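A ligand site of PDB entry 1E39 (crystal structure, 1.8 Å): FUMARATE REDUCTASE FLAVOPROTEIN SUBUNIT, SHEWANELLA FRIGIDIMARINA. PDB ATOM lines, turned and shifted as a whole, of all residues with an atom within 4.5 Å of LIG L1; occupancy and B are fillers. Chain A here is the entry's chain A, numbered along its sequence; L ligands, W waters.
The backbone NH (N) of Ala 5 is in hydrogen-bond range of the backbone carbonyl oxygen (O) of Ala 74, 2.6 Å away.
A carbon (C25) of LIG L1 is bonded to the side-chain sulfur of Cys 17 (1.8 Å). A carbon (C18) of LIG L1 is covalently linked to the side-chain sulfur (SG) of Cys 14, 1.9 Å away. NE2 of His 18 binds FE1 of LIG L1. A ring nitrogen (NE2) of His 75 is bound to an iron atom (FE1) of LIG L1, 2.0 Å away. NE2 of His 8 is bound to FE1 of LG2 L2, at 2.1 Å. An oxygen (O3) of LIG L1 lies within hydrogen-bond range of the backbone NH of His 75, 3.0 Å away. N of Ala 74 sits at hydrogen-bond distance from O4 of LIG L1 (2.8 Å).
Water W2 bridges an oxygen (O1) of LIG L1 (2.9 Å) and the backbone NH (N) of Leu 24 (2.9 Å).
ND1 of His 8 touches C26 of LIG L1 (3.97 Å). Val 9 touches LIG L1 (CG2 to C24, 3.9 Å). Leu 24 touches LIG L1 (CD1 to C11, 3.4 Å). Ser 73 touches LIG L1 (CA to O4, 3.6 Å). Of the 16 residues printed, 9 come within 4 Å of LIG L1.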
ATOM      1  N   ALA A   5      25.187   2.622  -2.882  1.00  0.00           N
ATOM      2  CA  ALA A   5      24.497   1.917  -3.972  1.00  0.00           C
ATOM      3  C   ALA A   5      23.870   2.926  -4.935  1.00  0.00           C
ATOM      4  O   ALA A   5      23.982   2.769  -6.147  1.00  0.00           O
ATOM      5  CB  ALA A   5      23.458   0.956  -3.423  1.00  0.00           C
ATOM      6  N   HIS A   8      26.289   4.164  -7.414  1.00  0.00           N
ATOM      7  CA  HIS A   8      26.679   3.283  -8.515  1.00  0.00           C
ATOM      8  C   HIS A   8      25.556   3.060  -9.526  1.00  0.00           C
ATOM      9  O   HIS A   8      25.790   2.853 -10.718  1.00  0.00           O
ATOM     10  CB  HIS A   8      27.140   1.934  -7.955  1.00  0.00           C
ATOM     11  CG  HIS A   8      28.503   1.968  -7.324  1.00  0.00           C
ATOM     12  ND1 HIS A   8      28.693   2.369  -6.026  1.00  0.00           N
ATOM     13  CD2 HIS A   8      29.734   1.647  -7.787  1.00  0.00           C
ATOM     14  CE1 HIS A   8      29.983   2.295  -5.739  1.00  0.00           C
ATOM     15  NE2 HIS A   8      30.651   1.860  -6.786  1.00  0.00           N
ATOM     16  N   VAL A   9      24.318   3.045  -9.037  1.00  0.00           N
ATOM     17  CA  VAL A   9      23.202   2.679  -9.915  1.00  0.00           C
ATOM     18  C   VAL A   9      22.918   3.776 -10.926  1.00  0.00           C
ATOM     19  O   VAL A   9      22.206   3.573 -11.917  1.00  0.00           O
ATOM     20  CB  VAL A   9      21.952   2.376  -9.085  1.00  0.00           C
ATOM     21  CG1 VAL A   9      20.716   2.248  -9.943  1.00  0.00           C
ATOM     22  CG2 VAL A   9      22.178   1.080  -8.291  1.00  0.00           C
ATOM     23  N   CYS A  14      21.832  -3.433 -11.071  1.00  0.00           N
ATOM     24  CA  CYS A  14      21.850  -4.134  -9.790  1.00  0.00           C
ATOM     25  C   CYS A  14      22.819  -5.311  -9.796  1.00  0.00           C
ATOM     26  O   CYS A  14      23.582  -5.481  -8.838  1.00  0.00           O
ATOM     27  CB  CYS A  14      20.443  -4.634  -9.452  1.00  0.00           C
ATOM     28  SG  CYS A  14      19.222  -3.308  -9.315  1.00  0.00           S
ATOM     29  N   SER A  16      25.509  -5.534 -11.189  1.00  0.00           N
ATOM     30  CA  SER A  16      26.950  -5.240 -11.184  1.00  0.00           C
ATOM     31  C   SER A  16      27.535  -5.637  -9.835  1.00  0.00           C
ATOM     32  O   SER A  16      28.709  -6.025  -9.703  1.00  0.00           O
ATOM     33  CB  SER A  16      27.209  -3.758 -11.471  1.00  0.00           C
ATOM     34  OG  SER A  16      26.638  -2.959 -10.451  1.00  0.00           O
ATOM     35  N   CYS A  17      26.715  -5.570  -8.777  1.00  0.00           N
ATOM     36  CA  CYS A  17      27.187  -6.071  -7.481  1.00  0.00           C
ATOM     37  C   CYS A  17      26.567  -7.402  -7.064  1.00  0.00           C
ATOM     38  O   CYS A  17      27.183  -8.228  -6.383  1.00  0.00           O
ATOM     39  CB  CYS A  17      26.887  -5.015  -6.411  1.00  0.00           C
ATOM     40  SG  CYS A  17      27.875  -3.526  -6.543  1.00  0.00           S
ATOM     41  N   HIS A  18      25.311  -7.620  -7.439  1.00  0.00           N
ATOM     42  CA  HIS A  18      24.538  -8.754  -6.939  1.00  0.00           C
ATOM     43  C   HIS A  18      24.585 -10.006  -7.801  1.00  0.00           C
ATOM     44  O   HIS A  18      24.966  -9.943  -8.960  1.00  0.00           O
ATOM     45  CB  HIS A  18      23.074  -8.288  -6.798  1.00  0.00           C
ATOM     46  CG  HIS A  18      22.829  -7.397  -5.628  1.00  0.00           C
ATOM     47  ND1 HIS A  18      22.829  -7.869  -4.330  1.00  0.00           N
ATOM     48  CD2 HIS A  18      22.552  -6.065  -5.528  1.00  0.00           C
ATOM     49  CE1 HIS A  18      22.572  -6.872  -3.507  1.00  0.00           C
ATOM     50  NE2 HIS A  18      22.400  -5.761  -4.194  1.00  0.00           N
ATOM     51  N   LEU A  24      21.743 -12.228  -1.300  1.00  0.00           N
ATOM     52  CA  LEU A  24      23.105 -12.108  -0.810  1.00  0.00           C
ATOM     53  C   LEU A  24      23.793 -13.459  -0.687  1.00  0.00           C
ATOM     54  O   LEU A  24      23.150 -14.389  -0.181  1.00  0.00           O
ATOM     55  CB  LEU A  24      23.071 -11.402   0.554  1.00  0.00           C
ATOM     56  CG  LEU A  24      22.374 -10.049   0.521  1.00  0.00           C
ATOM     57  CD1 LEU A  24      22.173  -9.491   1.918  1.00  0.00           C
ATOM     58  CD2 LEU A  24      23.191  -9.082  -0.331  1.00  0.00           C
ATOM     59  N   LEU A  29      29.468 -11.935   2.693  1.00  0.00           N
ATOM     60  CA  LEU A  29      29.253 -11.170   1.461  1.00  0.00           C
ATOM     61  C   LEU A  29      30.378 -11.481   0.481  1.00  0.00           C
ATOM     62  O   LEU A  29      30.962 -10.595  -0.157  1.00  0.00           O
ATOM     63  CB  LEU A  29      29.121  -9.677   1.774  1.00  0.00           C
ATOM     64  CG  LEU A  29      27.876  -9.272   2.571  1.00  0.00           C
ATOM     65  CD1 LEU A  29      27.902  -7.808   2.983  1.00  0.00           C
ATOM     66  CD2 LEU A  29      26.601  -9.566   1.786  1.00  0.00           C
ATOM     67  N   GLU A  32      29.651 -10.467  -3.351  1.00  0.00           N
ATOM     68  CA  GLU A  32      29.531  -9.017  -3.452  1.00  0.00           C
ATOM     69  C   GLU A  32      30.899  -8.351  -3.374  1.00  0.00           C
ATOM     70  O   GLU A  32      31.268  -7.559  -4.263  1.00  0.00           O
ATOM     71  CB  GLU A  32      28.530  -8.561  -2.372  1.00  0.00           C
ATOM     72  CG  GLU A  32      27.122  -9.117  -2.579  1.00  0.00           C
ATOM     73  CD  GLU A  32      26.892 -10.558  -2.200  1.00  0.00           C
ATOM     74  OE1 GLU A  32      27.811 -11.136  -1.564  1.00  0.00           O
ATOM     75  OE2 GLU A  32      25.835 -11.159  -2.512  1.00  0.00           O
ATOM     76  N   THR A  69      33.239  -4.487   2.466  1.00  0.00           N
ATOM     77  CA  THR A  69      32.010  -4.181   3.196  1.00  0.00           C
ATOM     78  C   THR A  69      32.232  -4.066   4.702  1.00  0.00           C
ATOM     79  O   THR A  69      31.295  -3.724   5.422  1.00  0.00           O
ATOM     80  CB  THR A  69      30.903  -5.196   2.893  1.00  0.00           C
ATOM     81  OG1 THR A  69      31.379  -6.531   3.060  1.00  0.00           O
ATOM     82  CG2 THR A  69      30.475  -5.054   1.435  1.00  0.00           C
ATOM     83  N   SER A  73      29.274   0.099   3.368  1.00  0.00           N
ATOM     84  CA  SER A  73      27.952  -0.506   3.147  1.00  0.00           C
ATOM     85  C   SER A  73      27.346   0.031   1.870  1.00  0.00           C
ATOM     86  O   SER A  73      27.754   1.083   1.351  1.00  0.00           O
ATOM     87  CB  SER A  73      26.982  -0.224   4.309  1.00  0.00           C
ATOM     88  OG  SER A  73      27.423  -0.883   5.482  1.00  0.00           O
ATOM     89  N   ALA A  74      26.358  -0.642   1.282  1.00  0.00           N
ATOM     90  CA  ALA A  74      25.881  -0.092   0.001  1.00  0.00           C
ATOM     91  C   ALA A  74      24.624   0.759   0.131  1.00  0.00           C
ATOM     92  O   ALA A  74      24.602   1.858  -0.414  1.00  0.00           O
ATOM     93  CB  ALA A  74      25.618  -1.239  -0.963  1.00  0.00           C
ATOM     94  N   HIS A  75      23.595   0.276   0.804  1.00  0.00           N
ATOM     95  CA  HIS A  75      22.293   0.930   0.815  1.00  0.00           C
ATOM     96  C   HIS A  75      22.081   1.787   2.046  1.00  0.00           C
ATOM     97  O   HIS A  75      20.997   2.343   2.244  1.00  0.00           O
ATOM     98  CB  HIS A  75      21.184  -0.138   0.665  1.00  0.00           C
ATOM     99  CG  HIS A  75      21.366  -0.935  -0.594  1.00  0.00           C
ATOM    100  ND1 HIS A  75      20.951  -0.485  -1.828  1.00  0.00           N
ATOM    101  CD2 HIS A  75      21.932  -2.141  -0.822  1.00  0.00           C
ATOM    102  CE1 HIS A  75      21.252  -1.391  -2.755  1.00  0.00           C
ATOM    103  NE2 HIS A  75      21.845  -2.427  -2.167  1.00  0.00           N
ATOM    104  N   GLU A  76      23.090   1.952   2.895  1.00  0.00           N
ATOM    105  CA  GLU A  76      22.998   2.860   4.038  1.00  0.00           C
ATOM    106  C   GLU A  76      24.369   3.450   4.339  1.00  0.00           C
ATOM    107  O   GLU A  76      25.374   2.841   3.937  1.00  0.00           O
ATOM    108  CB  GLU A  76      22.450   2.111   5.245  1.00  0.00           C
ATOM    109  CG  GLU A  76      23.413   1.083   5.820  1.00  0.00           C
ATOM    110  CD  GLU A  76      22.878   0.396   7.067  1.00  0.00           C
ATOM    111  OE1 GLU A  76      22.751   1.075   8.115  1.00  0.00           O
ATOM    112  OE2 GLU A  76      22.573  -0.811   7.037  1.00  0.00           O
ATOM    113  N   TYR A 298      23.555 -10.664   7.766  1.00  0.00           N
ATOM    114  CA  TYR A 298      22.842 -10.397   6.506  1.00  0.00           C
ATOM    115  C   TYR A 298      21.859 -11.508   6.161  1.00  0.00           C
ATOM    116  O   TYR A 298      20.911 -11.279   5.408  1.00  0.00           O
ATOM    117  CB  TYR A 298      23.850 -10.186   5.372  1.00  0.00           C
ATOM    118  CG  TYR A 298      24.854  -9.095   5.631  1.00  0.00           C
ATOM    119  CD1 TYR A 298      24.456  -7.760   5.550  1.00  0.00           C
ATOM    120  CD2 TYR A 298      26.181  -9.326   5.970  1.00  0.00           C
ATOM    121  CE1 TYR A 298      25.332  -6.732   5.781  1.00  0.00           C
ATOM    122  CE2 TYR A 298      27.069  -8.280   6.203  1.00  0.00           C
ATOM    123  CZ  TYR A 298      26.644  -6.974   6.111  1.00  0.00           C
ATOM    124  OH  TYR A 298      27.475  -5.901   6.336  1.00  0.00           O
HETATM  125 FE1  LIG L   1      22.107  -4.152  -3.123  1.00  0.00          FE
HETATM  126  C1  LIG L   1      21.903  -5.568  -0.056  1.00  0.00           C
HETATM  127  C2  LIG L   1      18.769  -4.580  -3.595  1.00  0.00           C
HETATM  128  C3  LIG L   1      22.264  -2.442  -6.059  1.00  0.00           C
HETATM  129  C4  LIG L   1      25.441  -3.979  -2.791  1.00  0.00           C
HETATM  130  N1  LIG L   1      20.665  -4.831  -2.073  1.00  0.00           N
HETATM  131  C5  LIG L   1      20.750  -5.377  -0.805  1.00  0.00           C
HETATM  132  C6  LIG L   1      19.479  -5.921  -0.380  1.00  0.00           C
HETATM  133  C7  LIG L   1      18.597  -5.722  -1.387  1.00  0.00           C
HETATM  134  C8  LIG L   1      19.339  -5.044  -2.427  1.00  0.00           C
HETATM  135  C9  LIG L   1      17.069  -5.832  -1.287  1.00  0.00           C
HETATM  136  C10 LIG L   1      19.249  -6.645   0.960  1.00  0.00           C
HETATM  137  C11 LIG L   1      19.186  -8.166   0.843  1.00  0.00           C
HETATM  138  C12 LIG L   1      18.745  -8.828   2.133  1.00  0.00           C
HETATM  139  O1  LIG L   1      18.498 -10.050   2.093  1.00  0.00           O
HETATM  140  O2  LIG L   1      18.649  -8.112   3.149  1.00  0.00           O
HETATM  141  N2  LIG L   1      20.796  -3.716  -4.619  1.00  0.00           N
HETATM  142  C13 LIG L   1      19.473  -4.091  -4.679  1.00  0.00           C
HETATM  143  C14 LIG L   1      18.872  -3.601  -5.901  1.00  0.00           C
HETATM  144  C15 LIG L   1      19.825  -2.924  -6.577  1.00  0.00           C
HETATM  145  C16 LIG L   1      21.024  -2.977  -5.752  1.00  0.00           C
HETATM  146  C17 LIG L   1      17.444  -3.944  -6.314  1.00  0.00           C
HETATM  147  C18 LIG L   1      19.689  -2.270  -7.800  1.00  0.00           C
HETATM  148  C19 LIG L   1      18.779  -1.130  -7.952  1.00  0.00           C
HETATM  149  N3  LIG L   1      23.525  -3.366  -4.175  1.00  0.00           N
HETATM  150  C20 LIG L   1      23.422  -2.591  -5.325  1.00  0.00           C
HETATM  151  C21 LIG L   1      24.715  -2.119  -5.768  1.00  0.00           C
HETATM  152  C22 LIG L   1      25.636  -2.592  -4.879  1.00  0.00           C
HETATM  153  C23 LIG L   1      24.885  -3.328  -3.892  1.00  0.00           C
HETATM  154  C24 LIG L   1      25.019  -1.369  -7.053  1.00  0.00           C
HETATM  155  C25 LIG L   1      27.019  -2.674  -5.148  1.00  0.00           C
HETATM  156  C26 LIG L   1      27.795  -1.428  -5.284  1.00  0.00           C
HETATM  157  N4  LIG L   1      23.415  -4.650  -1.686  1.00  0.00           N
HETATM  158  C27 LIG L   1      24.776  -4.749  -1.867  1.00  0.00           C
HETATM  159  C28 LIG L   1      25.400  -5.298  -0.681  1.00  0.00           C
HETATM  160  C29 LIG L   1      24.413  -5.559   0.209  1.00  0.00           C
HETATM  161  C30 LIG L   1      23.164  -5.173  -0.433  1.00  0.00           C
HETATM  162  C31 LIG L   1      26.874  -5.077  -0.311  1.00  0.00           C
HETATM  163  C32 LIG L   1      24.595  -5.724   1.726  1.00  0.00           C
HETATM  164  C33 LIG L   1      23.922  -4.666   2.601  1.00  0.00           C
HETATM  165  C34 LIG L   1      24.509  -3.280   2.370  1.00  0.00           C
HETATM  166  O3  LIG L   1      23.758  -2.285   2.303  1.00  0.00           O
HETATM  167  O4  LIG L   1      25.749  -3.164   2.265  1.00  0.00           O
HETATM  168 FE1  LG2 L   2      32.675   1.363  -6.934  1.00  0.00          FE
HETATM  169  C1  LG2 L   2      32.888   4.693  -7.230  1.00  0.00           C
HETATM  170  C2  LG2 L   2      33.283   1.546  -3.580  1.00  0.00           C
HETATM  171  C3  LG2 L   2      31.563  -1.818  -6.523  1.00  0.00           C
HETATM  172  C4  LG2 L   2      33.008   0.951 -10.172  1.00  0.00           C
HETATM  173  N1  LG2 L   2      32.907   2.767  -5.692  1.00  0.00           N
HETATM  174  C5  LG2 L   2      32.904   4.128  -5.958  1.00  0.00           C
HETATM  175  C6  LG2 L   2      33.281   4.911  -4.803  1.00  0.00           C
HETATM  176  C7  LG2 L   2      33.558   4.010  -3.822  1.00  0.00           C
HETATM  177  C8  LG2 L   2      33.355   2.681  -4.372  1.00  0.00           C
HETATM  178  C9  LG2 L   2      33.833   4.299  -2.351  1.00  0.00           C
HETATM  179  C10 LG2 L   2      33.129   6.434  -4.695  1.00  0.00           C
HETATM  180  C11 LG2 L   2      31.745   7.013  -4.407  1.00  0.00           C
HETATM  181  C12 LG2 L   2      31.655   8.526  -4.423  1.00  0.00           C
HETATM  182  O1  LG2 L   2      30.671   9.104  -3.917  1.00  0.00           O
HETATM  183  O2  LG2 L   2      32.595   9.168  -4.953  1.00  0.00           O
HETATM  184  N2  LG2 L   2      32.540   0.069  -5.309  1.00  0.00           N
HETATM  185  C13 LG2 L   2      32.883   0.301  -4.007  1.00  0.00           C
HETATM  186  C14 LG2 L   2      32.596  -0.896  -3.237  1.00  0.00           C
HETATM  187  C15 LG2 L   2      32.094  -1.837  -4.072  1.00  0.00           C
HETATM  188  C16 LG2 L   2      32.058  -1.211  -5.391  1.00  0.00           C
HETATM  189  C17 LG2 L   2      32.973  -1.108  -1.764  1.00  0.00           C
HETATM  190  C18 LG2 L   2      31.431  -3.035  -3.786  1.00  0.00           C
HETATM  191  C19 LG2 L   2      30.416  -3.125  -2.730  1.00  0.00           C
HETATM  192  N3  LG2 L   2      32.305  -0.084  -8.039  1.00  0.00           N
HETATM  193  C20 LG2 L   2      31.702  -1.310  -7.798  1.00  0.00           C
HETATM  194  C21 LG2 L   2      31.554  -2.086  -9.008  1.00  0.00           C
HETATM  195  C22 LG2 L   2      32.049  -1.336 -10.020  1.00  0.00           C
HETATM  196  C23 LG2 L   2      32.490  -0.093  -9.412  1.00  0.00           C
HETATM  197  C24 LG2 L   2      31.006  -3.506  -9.126  1.00  0.00           C
HETATM  198  C25 LG2 L   2      32.327  -1.713 -11.334  1.00  0.00           C
HETATM  199  C26 LG2 L   2      31.278  -2.265 -12.177  1.00  0.00           C
HETATM  200  N4  LG2 L   2      32.737   2.624  -8.454  1.00  0.00           N
HETATM  201  C27 LG2 L   2      32.956   2.262  -9.757  1.00  0.00           C
HETATM  202  C28 LG2 L   2      33.269   3.420 -10.570  1.00  0.00           C
HETATM  203  C29 LG2 L   2      33.245   4.493  -9.730  1.00  0.00           C
HETATM  204  C30 LG2 L   2      32.949   3.982  -8.410  1.00  0.00           C
HETATM  205  C31 LG2 L   2      33.426   3.429 -12.093  1.00  0.00           C
HETATM  206  C32 LG2 L   2      33.673   5.924 -10.055  1.00  0.00           C
HETATM  207  C33 LG2 L   2      35.194   6.150 -10.002  1.00  0.00           C
HETATM  208  C34 LG2 L   2      35.913   5.329 -11.063  1.00  0.00           C
HETATM  209  O3  LG2 L   2      36.443   4.249 -10.725  1.00  0.00           O
HETATM  210  O4  LG2 L   2      35.916   5.764 -12.240  1.00  0.00           O
HETATM  211  O   HOH W   1      28.091  -4.928  -3.889  1.00  0.00           O
HETATM  212  O   HOH W   2      19.289 -12.024   0.188  1.00  0.00           O
HETATM  213  O   HOH W   3      19.181  -7.888  -4.447  1.00  0.00           O
